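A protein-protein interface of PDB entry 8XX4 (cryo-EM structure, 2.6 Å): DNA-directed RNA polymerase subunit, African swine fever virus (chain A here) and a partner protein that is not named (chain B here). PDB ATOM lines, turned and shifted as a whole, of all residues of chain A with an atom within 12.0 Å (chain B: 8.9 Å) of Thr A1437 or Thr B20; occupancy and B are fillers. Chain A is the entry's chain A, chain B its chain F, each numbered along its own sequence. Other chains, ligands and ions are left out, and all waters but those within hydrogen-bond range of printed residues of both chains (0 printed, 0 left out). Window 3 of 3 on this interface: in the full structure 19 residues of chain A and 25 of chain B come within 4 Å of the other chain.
The side-chain carboxylate of Glu A1433 is in salt-bridge range of the guanidinium group of Arg B53 (2.8 Å).
The side-chain hydroxyl of Thr A1437 is in hydrogen-bond range of the backbone carbonyl oxygen of Cys B19 (3.2 Å).
The backbone carbonyl oxygen (O) of Pro B15 sits at hydrogen-bond distance from the side-chain sulfur (SG) of Cys B19, 3.4 Å away.
The backbone carbonyl oxygen of Asn B17 sits at hydrogen-bond distance from the side-chain hydroxyl of Thr B20 (2.7 Å).
Met A1431 touches Pro B15 (SD to CB, 3.5 Å).
CB of Met A1431 touches SG of Cys B19 (3.5 Å).
Cys B19 touches Glu A1433 (SG to CG, 3.6 Å).
Glu A1433 touches Val B22.
Thr B16 touches Ile A1436 (O to CG2, 3.3 Å).
CB of Cys B19 touches CD1 of Ile A1436, at 3.7 Å.
CG2 of Ile A1436 touches CG2 of Thr B20, at 3.8 Å.
Thr A1437 touches Thr B20.
Tyr A1440 touches Thr B20 (O to CG2, 3.2 Å).
Thr A1437 touches two residues of chain B.
Of the printed residues of chain A, Thr B20 touches Ile A1436, Thr A1437 and Tyr A1440.
Asn B17 touches none of the printed residues of chain A.
Printed residues of chain A within 4 Å of Cys B19: Met A1431 (3.5 Å), Glu A1433 (3.6 Å), Ile A1436 (3.7 Å) and Thr A1437 (3.2 Å).
Printed residues of chain B within 4 Å of Met A1431: Pro B15 (3.5 Å) and Cys B19 (3.5 Å).
Of the printed residues of chain A, Pro B15 touches Met A1431 (3.5 Å).
Of the printed residues of chain B, Glu A1433 touches Cys B19, Val B22 and Arg B53.
Of the printed residues of chain B, Ile A1436 touches Thr B16, Cys B19 and Thr B20.
Glu B23 touches none of the printed residues of chain A.
Lys A1434 touches none of the printed residues of chain B.
The nearest residue of chain B that does not touch Thr A1437 is Asn B21 (4.9 Å).
The nearest residue of chain A that does not touch Thr B20 is Lys A1441 (4.5 Å).
Hydrophobic or aromatic side chains of chain A within 4 Å of the printed part of chain B: Met A1431 and Ile A1436.
Of the 15 printed residues of chain B, 6 touch a printed residue of chain A.
Hydrophobic or aromatic side chains of chain B within 4 Å of the printed part of chain A: Pro B15 and Val B22.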
ATOM      1  N   ILE A1430      -5.565  -1.340 -21.715  1.00  0.00           N
ATOM      2  CA  ILE A1430      -4.556  -2.083 -20.985  1.00  0.00           C
ATOM      3  C   ILE A1430      -5.230  -2.707 -19.773  1.00  0.00           C
ATOM      4  O   ILE A1430      -6.275  -2.253 -19.308  1.00  0.00           O
ATOM      5  CB  ILE A1430      -3.365  -1.196 -20.574  1.00  0.00           C
ATOM      6  CG1 ILE A1430      -3.727  -0.337 -19.371  1.00  0.00           C
ATOM      7  CG2 ILE A1430      -2.953  -0.308 -21.721  1.00  0.00           C
ATOM      8  CD1 ILE A1430      -2.636   0.602 -18.950  1.00  0.00           C
ATOM      9  N   MET A1431      -4.628  -3.776 -19.270  1.00  0.00           N
ATOM     10  CA  MET A1431      -5.188  -4.527 -18.157  1.00  0.00           C
ATOM     11  C   MET A1431      -4.807  -3.851 -16.849  1.00  0.00           C
ATOM     12  O   MET A1431      -3.668  -3.402 -16.686  1.00  0.00           O
ATOM     13  CB  MET A1431      -4.697  -5.975 -18.170  1.00  0.00           C
ATOM     14  CG  MET A1431      -4.922  -6.696 -19.482  1.00  0.00           C
ATOM     15  SD  MET A1431      -6.545  -7.450 -19.682  1.00  0.00           S
ATOM     16  CE  MET A1431      -7.020  -7.774 -18.001  1.00  0.00           C
ATOM     17  N   ASP A1432      -5.763  -3.768 -15.927  1.00  0.00           N
ATOM     18  CA  ASP A1432      -5.525  -3.154 -14.627  1.00  0.00           C
ATOM     19  C   ASP A1432      -4.811  -4.125 -13.699  1.00  0.00           C
ATOM     20  O   ASP A1432      -5.455  -4.880 -12.968  1.00  0.00           O
ATOM     21  CB  ASP A1432      -6.840  -2.696 -14.004  1.00  0.00           C
ATOM     22  CG  ASP A1432      -6.666  -1.520 -13.081  1.00  0.00           C
ATOM     23  OD1 ASP A1432      -5.527  -1.262 -12.644  1.00  0.00           O
ATOM     24  OD2 ASP A1432      -7.673  -0.846 -12.791  1.00  0.00           O
ATOM     25  N   GLU A1433      -3.478  -4.100 -13.711  1.00  0.00           N
ATOM     26  CA  GLU A1433      -2.709  -5.086 -12.961  1.00  0.00           C
ATOM     27  C   GLU A1433      -2.950  -4.972 -11.462  1.00  0.00           C
ATOM     28  O   GLU A1433      -3.089  -5.988 -10.773  1.00  0.00           O
ATOM     29  CB  GLU A1433      -1.225  -4.937 -13.278  1.00  0.00           C
ATOM     30  CG  GLU A1433      -0.814  -5.639 -14.550  1.00  0.00           C
ATOM     31  CD  GLU A1433       0.010  -4.762 -15.461  1.00  0.00           C
ATOM     32  OE1 GLU A1433       0.478  -3.700 -15.003  1.00  0.00           O
ATOM     33  OE2 GLU A1433       0.196  -5.136 -16.636  1.00  0.00           O
ATOM     34  N   LYS A1434      -2.990  -3.751 -10.933  1.00  0.00           N
ATOM     35  CA  LYS A1434      -3.220  -3.576  -9.504  1.00  0.00           C
ATOM     36  C   LYS A1434      -4.585  -4.115  -9.101  1.00  0.00           C
ATOM     37  O   LYS A1434      -4.714  -4.855  -8.118  1.00  0.00           O
ATOM     38  CB  LYS A1434      -3.088  -2.097  -9.137  1.00  0.00           C
ATOM     39  CG  LYS A1434      -3.384  -1.778  -7.683  1.00  0.00           C
ATOM     40  CD  LYS A1434      -3.106  -0.313  -7.384  1.00  0.00           C
ATOM     41  CE  LYS A1434      -4.307   0.364  -6.748  1.00  0.00           C
ATOM     42  NZ  LYS A1434      -3.931   1.624  -6.052  1.00  0.00           N
ATOM     43  N   TYR A1435      -5.613  -3.770  -9.875  1.00  0.00           N
ATOM     44  CA  TYR A1435      -6.969  -4.196  -9.559  1.00  0.00           C
ATOM     45  C   TYR A1435      -7.112  -5.708  -9.648  1.00  0.00           C
ATOM     46  O   TYR A1435      -7.734  -6.331  -8.783  1.00  0.00           O
ATOM     47  CB  TYR A1435      -7.948  -3.504 -10.501  1.00  0.00           C
ATOM     48  CG  TYR A1435      -9.399  -3.684 -10.151  1.00  0.00           C
ATOM     49  CD1 TYR A1435      -9.964  -2.987  -9.099  1.00  0.00           C
ATOM     50  CD2 TYR A1435     -10.210  -4.528 -10.888  1.00  0.00           C
ATOM     51  CE1 TYR A1435     -11.285  -3.136  -8.779  1.00  0.00           C
ATOM     52  CE2 TYR A1435     -11.535  -4.683 -10.575  1.00  0.00           C
ATOM     53  CZ  TYR A1435     -12.067  -3.984  -9.519  1.00  0.00           C
ATOM     54  OH  TYR A1435     -13.391  -4.128  -9.199  1.00  0.00           O
ATOM     55  N   ILE A1436      -6.540  -6.319 -10.685  1.00  0.00           N
ATOM     56  CA  ILE A1436      -6.656  -7.765 -10.843  1.00  0.00           C
ATOM     57  C   ILE A1436      -5.872  -8.485  -9.758  1.00  0.00           C
ATOM     58  O   ILE A1436      -6.311  -9.515  -9.235  1.00  0.00           O
ATOM     59  CB  ILE A1436      -6.201  -8.185 -12.250  1.00  0.00           C
ATOM     60  CG1 ILE A1436      -7.105  -7.559 -13.302  1.00  0.00           C
ATOM     61  CG2 ILE A1436      -6.243  -9.685 -12.396  1.00  0.00           C
ATOM     62  CD1 ILE A1436      -6.439  -7.389 -14.624  1.00  0.00           C
ATOM     63  N   THR A1437      -4.699  -7.959  -9.401  1.00  0.00           N
ATOM     64  CA  THR A1437      -3.916  -8.565  -8.332  1.00  0.00           C
ATOM     65  C   THR A1437      -4.659  -8.510  -7.005  1.00  0.00           C
ATOM     66  O   THR A1437      -4.657  -9.484  -6.245  1.00  0.00           O
ATOM     67  CB  THR A1437      -2.563  -7.868  -8.212  1.00  0.00           C
ATOM     68  OG1 THR A1437      -2.058  -7.575  -9.518  1.00  0.00           O
ATOM     69  CG2 THR A1437      -1.575  -8.753  -7.480  1.00  0.00           C
ATOM     70  N   GLU A1438      -5.308  -7.388  -6.710  1.00  0.00           N
ATOM     71  CA  GLU A1438      -5.970  -7.237  -5.423  1.00  0.00           C
ATOM     72  C   GLU A1438      -7.412  -7.727  -5.416  1.00  0.00           C
ATOM     73  O   GLU A1438      -8.042  -7.716  -4.354  1.00  0.00           O
ATOM     74  CB  GLU A1438      -5.922  -5.774  -4.978  1.00  0.00           C
ATOM     75  CG  GLU A1438      -6.911  -4.877  -5.678  1.00  0.00           C
ATOM     76  CD  GLU A1438      -6.467  -3.432  -5.692  1.00  0.00           C
ATOM     77  OE1 GLU A1438      -5.322  -3.161  -5.273  1.00  0.00           O
ATOM     78  OE2 GLU A1438      -7.257  -2.568  -6.124  1.00  0.00           O
ATOM     79  N   ASN A1439      -7.953  -8.153  -6.552  1.00  0.00           N
ATOM     80  CA  ASN A1439      -9.333  -8.621  -6.609  1.00  0.00           C
ATOM     81  C   ASN A1439      -9.493 -10.006  -7.214  1.00  0.00           C
ATOM     82  O   ASN A1439     -10.314 -10.787  -6.732  1.00  0.00           O
ATOM     83  CB  ASN A1439     -10.188  -7.629  -7.404  1.00  0.00           C
ATOM     84  CG  ASN A1439     -10.629  -6.446  -6.576  1.00  0.00           C
ATOM     85  OD1 ASN A1439     -11.542  -6.551  -5.760  1.00  0.00           O
ATOM     86  ND2 ASN A1439      -9.982  -5.308  -6.782  1.00  0.00           N
ATOM     87  N   TYR A1440      -8.745 -10.332  -8.263  1.00  0.00           N
ATOM     88  CA  TYR A1440      -8.902 -11.610  -8.956  1.00  0.00           C
ATOM     89  C   TYR A1440      -7.824 -12.587  -8.490  1.00  0.00           C
ATOM     90  O   TYR A1440      -6.887 -12.927  -9.209  1.00  0.00           O
ATOM     91  CB  TYR A1440      -8.862 -11.403 -10.467  1.00  0.00           C
ATOM     92  CG  TYR A1440     -10.037 -10.624 -11.005  1.00  0.00           C
ATOM     93  CD1 TYR A1440     -10.040  -9.237 -10.993  1.00  0.00           C
ATOM     94  CD2 TYR A1440     -11.146 -11.274 -11.524  1.00  0.00           C
ATOM     95  CE1 TYR A1440     -11.112  -8.522 -11.478  1.00  0.00           C
ATOM     96  CE2 TYR A1440     -12.224 -10.565 -12.013  1.00  0.00           C
ATOM     97  CZ  TYR A1440     -12.201  -9.190 -11.987  1.00  0.00           C
ATOM     98  OH  TYR A1440     -13.270  -8.475 -12.472  1.00  0.00           O
ATOM     99  N   LYS A1441      -7.982 -13.040  -7.253  1.00  0.00           N
ATOM    100  CA  LYS A1441      -7.026 -13.964  -6.658  1.00  0.00           C
ATOM    101  C   LYS A1441      -7.110 -15.340  -7.311  1.00  0.00           C
ATOM    102  O   LYS A1441      -6.405 -15.621  -8.282  1.00  0.00           O
ATOM    103  CB  LYS A1441      -7.262 -14.078  -5.152  1.00  0.00           C
ATOM    104  CG  LYS A1441      -7.214 -12.748  -4.420  1.00  0.00           C
ATOM    105  CD  LYS A1441      -8.460 -12.539  -3.582  1.00  0.00           C
ATOM    106  CE  LYS A1441      -8.650 -11.074  -3.233  1.00  0.00           C
ATOM    107  NZ  LYS A1441     -10.088 -10.690  -3.217  1.00  0.00           N
ATOM    108  N   ILE B  12       0.021 -12.884 -24.598  1.00  0.00           N
ATOM    109  CA  ILE B  12      -0.638 -13.278 -23.365  1.00  0.00           C
ATOM    110  C   ILE B  12      -2.031 -13.768 -23.722  1.00  0.00           C
ATOM    111  O   ILE B  12      -2.923 -12.967 -24.025  1.00  0.00           O
ATOM    112  CB  ILE B  12      -0.690 -12.128 -22.358  1.00  0.00           C
ATOM    113  CG1 ILE B  12       0.727 -11.714 -21.977  1.00  0.00           C
ATOM    114  CG2 ILE B  12      -1.451 -12.548 -21.145  1.00  0.00           C
ATOM    115  CD1 ILE B  12       0.855 -10.276 -21.610  1.00  0.00           C
ATOM    116  N   ASP B  14      -4.217 -15.424 -21.810  1.00  0.00           N
ATOM    117  CA  ASP B  14      -5.189 -15.220 -20.737  1.00  0.00           C
ATOM    118  C   ASP B  14      -4.764 -13.987 -19.956  1.00  0.00           C
ATOM    119  O   ASP B  14      -4.155 -14.097 -18.885  1.00  0.00           O
ATOM    120  CB  ASP B  14      -5.290 -16.445 -19.830  1.00  0.00           C
ATOM    121  CG  ASP B  14      -6.613 -16.518 -19.103  1.00  0.00           C
ATOM    122  OD1 ASP B  14      -7.519 -15.730 -19.443  1.00  0.00           O
ATOM    123  OD2 ASP B  14      -6.749 -17.362 -18.194  1.00  0.00           O
ATOM    124  N   PRO B  15      -5.056 -12.794 -20.473  1.00  0.00           N
ATOM    125  CA  PRO B  15      -4.566 -11.571 -19.817  1.00  0.00           C
ATOM    126  C   PRO B  15      -5.098 -11.365 -18.411  1.00  0.00           C
ATOM    127  O   PRO B  15      -4.413 -10.744 -17.591  1.00  0.00           O
ATOM    128  CB  PRO B  15      -5.024 -10.460 -20.770  1.00  0.00           C
ATOM    129  CG  PRO B  15      -6.131 -11.055 -21.547  1.00  0.00           C
ATOM    130  CD  PRO B  15      -5.833 -12.501 -21.687  1.00  0.00           C
ATOM    131  N   THR B  16      -6.300 -11.854 -18.104  1.00  0.00           N
ATOM    132  CA  THR B  16      -6.840 -11.692 -16.759  1.00  0.00           C
ATOM    133  C   THR B  16      -6.028 -12.482 -15.742  1.00  0.00           C
ATOM    134  O   THR B  16      -5.612 -11.943 -14.712  1.00  0.00           O
ATOM    135  CB  THR B  16      -8.301 -12.131 -16.723  1.00  0.00           C
ATOM    136  OG1 THR B  16      -8.938 -11.780 -17.957  1.00  0.00           O
ATOM    137  CG2 THR B  16      -9.021 -11.454 -15.577  1.00  0.00           C
ATOM    138  N   ASN B  17      -5.795 -13.766 -16.018  1.00  0.00           N
ATOM    139  CA  ASN B  17      -5.034 -14.597 -15.094  1.00  0.00           C
ATOM    140  C   ASN B  17      -3.566 -14.203 -15.070  1.00  0.00           C
ATOM    141  O   ASN B  17      -2.918 -14.293 -14.023  1.00  0.00           O
ATOM    142  CB  ASN B  17      -5.191 -16.068 -15.474  1.00  0.00           C
ATOM    143  CG  ASN B  17      -4.060 -16.928 -14.961  1.00  0.00           C
ATOM    144  OD1 ASN B  17      -3.947 -17.172 -13.761  1.00  0.00           O
ATOM    145  ND2 ASN B  17      -3.215 -17.396 -15.868  1.00  0.00           N
ATOM    146  N   PHE B  18      -3.036 -13.756 -16.206  1.00  0.00           N
ATOM    147  CA  PHE B  18      -1.640 -13.343 -16.279  1.00  0.00           C
ATOM    148  C   PHE B  18      -1.358 -12.175 -15.348  1.00  0.00           C
ATOM    149  O   PHE B  18      -0.306 -12.124 -14.703  1.00  0.00           O
ATOM    150  CB  PHE B  18      -1.302 -12.980 -17.721  1.00  0.00           C
ATOM    151  CG  PHE B  18       0.138 -12.636 -17.955  1.00  0.00           C
ATOM    152  CD1 PHE B  18       1.048 -13.615 -18.300  1.00  0.00           C
ATOM    153  CD2 PHE B  18       0.573 -11.328 -17.870  1.00  0.00           C
ATOM    154  CE1 PHE B  18       2.365 -13.297 -18.530  1.00  0.00           C
ATOM    155  CE2 PHE B  18       1.887 -11.009 -18.097  1.00  0.00           C
ATOM    156  CZ  PHE B  18       2.784 -11.993 -18.427  1.00  0.00           C
ATOM    157  N   CYS B  19      -2.288 -11.230 -15.260  1.00  0.00           N
ATOM    158  CA  CYS B  19      -2.081 -10.018 -14.481  1.00  0.00           C
ATOM    159  C   CYS B  19      -2.242 -10.231 -12.984  1.00  0.00           C
ATOM    160  O   CYS B  19      -1.980  -9.301 -12.215  1.00  0.00           O
ATOM    161  CB  CYS B  19      -3.039  -8.928 -14.958  1.00  0.00           C
ATOM    162  SG  CYS B  19      -2.509  -8.137 -16.482  1.00  0.00           S
ATOM    163  N   THR B  20      -2.672 -11.417 -12.553  1.00  0.00           N
ATOM    164  CA  THR B  20      -2.734 -11.702 -11.124  1.00  0.00           C
ATOM    165  C   THR B  20      -1.342 -11.714 -10.509  1.00  0.00           C
ATOM    166  O   THR B  20      -1.157 -11.293  -9.363  1.00  0.00           O
ATOM    167  CB  THR B  20      -3.445 -13.033 -10.885  1.00  0.00           C
ATOM    168  OG1 THR B  20      -2.640 -14.107 -11.386  1.00  0.00           O
ATOM    169  CG2 THR B  20      -4.784 -13.046 -11.589  1.00  0.00           C
ATOM    170  N   ASN B  21      -0.350 -12.204 -11.251  1.00  0.00           N
ATOM    171  CA  ASN B  21       1.057 -12.143 -10.844  1.00  0.00           C
ATOM    172  C   ASN B  21       1.865 -11.894 -12.115  1.00  0.00           C
ATOM    173  O   ASN B  21       2.253 -12.838 -12.804  1.00  0.00           O
ATOM    174  CB  ASN B  21       1.490 -13.419 -10.135  1.00  0.00           C
ATOM    175  CG  ASN B  21       1.073 -13.448  -8.678  1.00  0.00           C
ATOM    176  OD1 ASN B  21       0.324 -14.325  -8.252  1.00  0.00           O
ATOM    177  ND2 ASN B  21       1.566 -12.491  -7.903  1.00  0.00           N
ATOM    178  N   VAL B  22       2.110 -10.620 -12.420  1.00  0.00           N
ATOM    179  CA  VAL B  22       2.753 -10.282 -13.686  1.00  0.00           C
ATOM    180  C   VAL B  22       4.221 -10.690 -13.683  1.00  0.00           C
ATOM    181  O   VAL B  22       4.726 -11.214 -14.677  1.00  0.00           O
ATOM    182  CB  VAL B  22       2.581  -8.786 -13.999  1.00  0.00           C
ATOM    183  CG1 VAL B  22       3.642  -8.325 -14.976  1.00  0.00           C
ATOM    184  CG2 VAL B  22       1.214  -8.544 -14.581  1.00  0.00           C
ATOM    185  N   GLU B  23       4.931 -10.453 -12.581  1.00  0.00           N
ATOM    186  CA  GLU B  23       6.361 -10.749 -12.560  1.00  0.00           C
ATOM    187  C   GLU B  23       6.619 -12.248 -12.661  1.00  0.00           C
ATOM    188  O   GLU B  23       7.451 -12.694 -13.462  1.00  0.00           O
ATOM    189  CB  GLU B  23       7.000 -10.173 -11.298  1.00  0.00           C
ATOM    190  CG  GLU B  23       7.369  -8.699 -11.398  1.00  0.00           C
ATOM    191  CD  GLU B  23       8.399  -8.413 -12.483  1.00  0.00           C
ATOM    192  OE1 GLU B  23       9.590  -8.240 -12.144  1.00  0.00           O
ATOM    193  OE2 GLU B  23       8.017  -8.336 -13.670  1.00  0.00           O
ATOM    194  N   ALA B  24       5.906 -13.044 -11.863  1.00  0.00           N
ATOM    195  CA  ALA B  24       6.100 -14.489 -11.886  1.00  0.00           C
ATOM    196  C   ALA B  24       5.729 -15.071 -13.242  1.00  0.00           C
ATOM    197  O   ALA B  24       6.486 -15.856 -13.824  1.00  0.00           O
ATOM    198  CB  ALA B  24       5.277 -15.144 -10.778  1.00  0.00           C
ATOM    199  N   HIS B  25       4.561 -14.691 -13.761  1.00  0.00           N
ATOM    200  CA  HIS B  25       4.113 -15.210 -15.047  1.00  0.00           C
ATOM    201  C   HIS B  25       5.032 -14.764 -16.173  1.00  0.00           C
ATOM    202  O   HIS B  25       5.303 -15.529 -17.103  1.00  0.00           O
ATOM    203  CB  HIS B  25       2.678 -14.766 -15.311  1.00  0.00           C
ATOM    204  CG  HIS B  25       1.674 -15.404 -14.405  1.00  0.00           C
ATOM    205  ND1 HIS B  25       0.646 -14.699 -13.821  1.00  0.00           N
ATOM    206  CD2 HIS B  25       1.540 -16.683 -13.984  1.00  0.00           C
ATOM    207  CE1 HIS B  25      -0.079 -15.516 -13.079  1.00  0.00           C
ATOM    208  NE2 HIS B  25       0.443 -16.726 -13.159  1.00  0.00           N
ATOM    209  N   LYS B  28       8.133 -16.895 -16.008  1.00  0.00           N
ATOM    210  CA  LYS B  28       7.827 -18.237 -16.495  1.00  0.00           C
ATOM    211  C   LYS B  28       7.741 -18.260 -18.016  1.00  0.00           C
ATOM    212  O   LYS B  28       8.307 -19.141 -18.671  1.00  0.00           O
ATOM    213  CB  LYS B  28       6.517 -18.735 -15.883  1.00  0.00           C
ATOM    214  CG  LYS B  28       6.574 -19.014 -14.395  1.00  0.00           C
ATOM    215  CD  LYS B  28       5.185 -18.937 -13.777  1.00  0.00           C
ATOM    216  CE  LYS B  28       4.947 -20.064 -12.790  1.00  0.00           C
ATOM    217  NZ  LYS B  28       4.338 -19.570 -11.524  1.00  0.00           N
ATOM    218  N   ARG B  53       9.384  -3.437 -18.746  1.00  0.00           N
ATOM    219  CA  ARG B  53       8.268  -4.079 -19.418  1.00  0.00           C
ATOM    220  C   ARG B  53       7.245  -3.011 -19.774  1.00  0.00           C
ATOM    221  O   ARG B  53       7.465  -1.815 -19.573  1.00  0.00           O
ATOM    222  CB  ARG B  53       7.666  -5.190 -18.551  1.00  0.00           C
ATOM    223  CG  ARG B  53       7.392  -4.773 -17.131  1.00  0.00           C
ATOM    224  CD  ARG B  53       6.432  -5.724 -16.465  1.00  0.00           C
ATOM    225  NE  ARG B  53       5.053  -5.312 -16.674  1.00  0.00           N
ATOM    226  CZ  ARG B  53       4.219  -4.978 -15.701  1.00  0.00           C
ATOM    227  NH1 ARG B  53       4.592  -5.000 -14.434  1.00  0.00           N
ATOM    228  NH2 ARG B  53       2.981  -4.609 -16.009  1.00  0.00           N
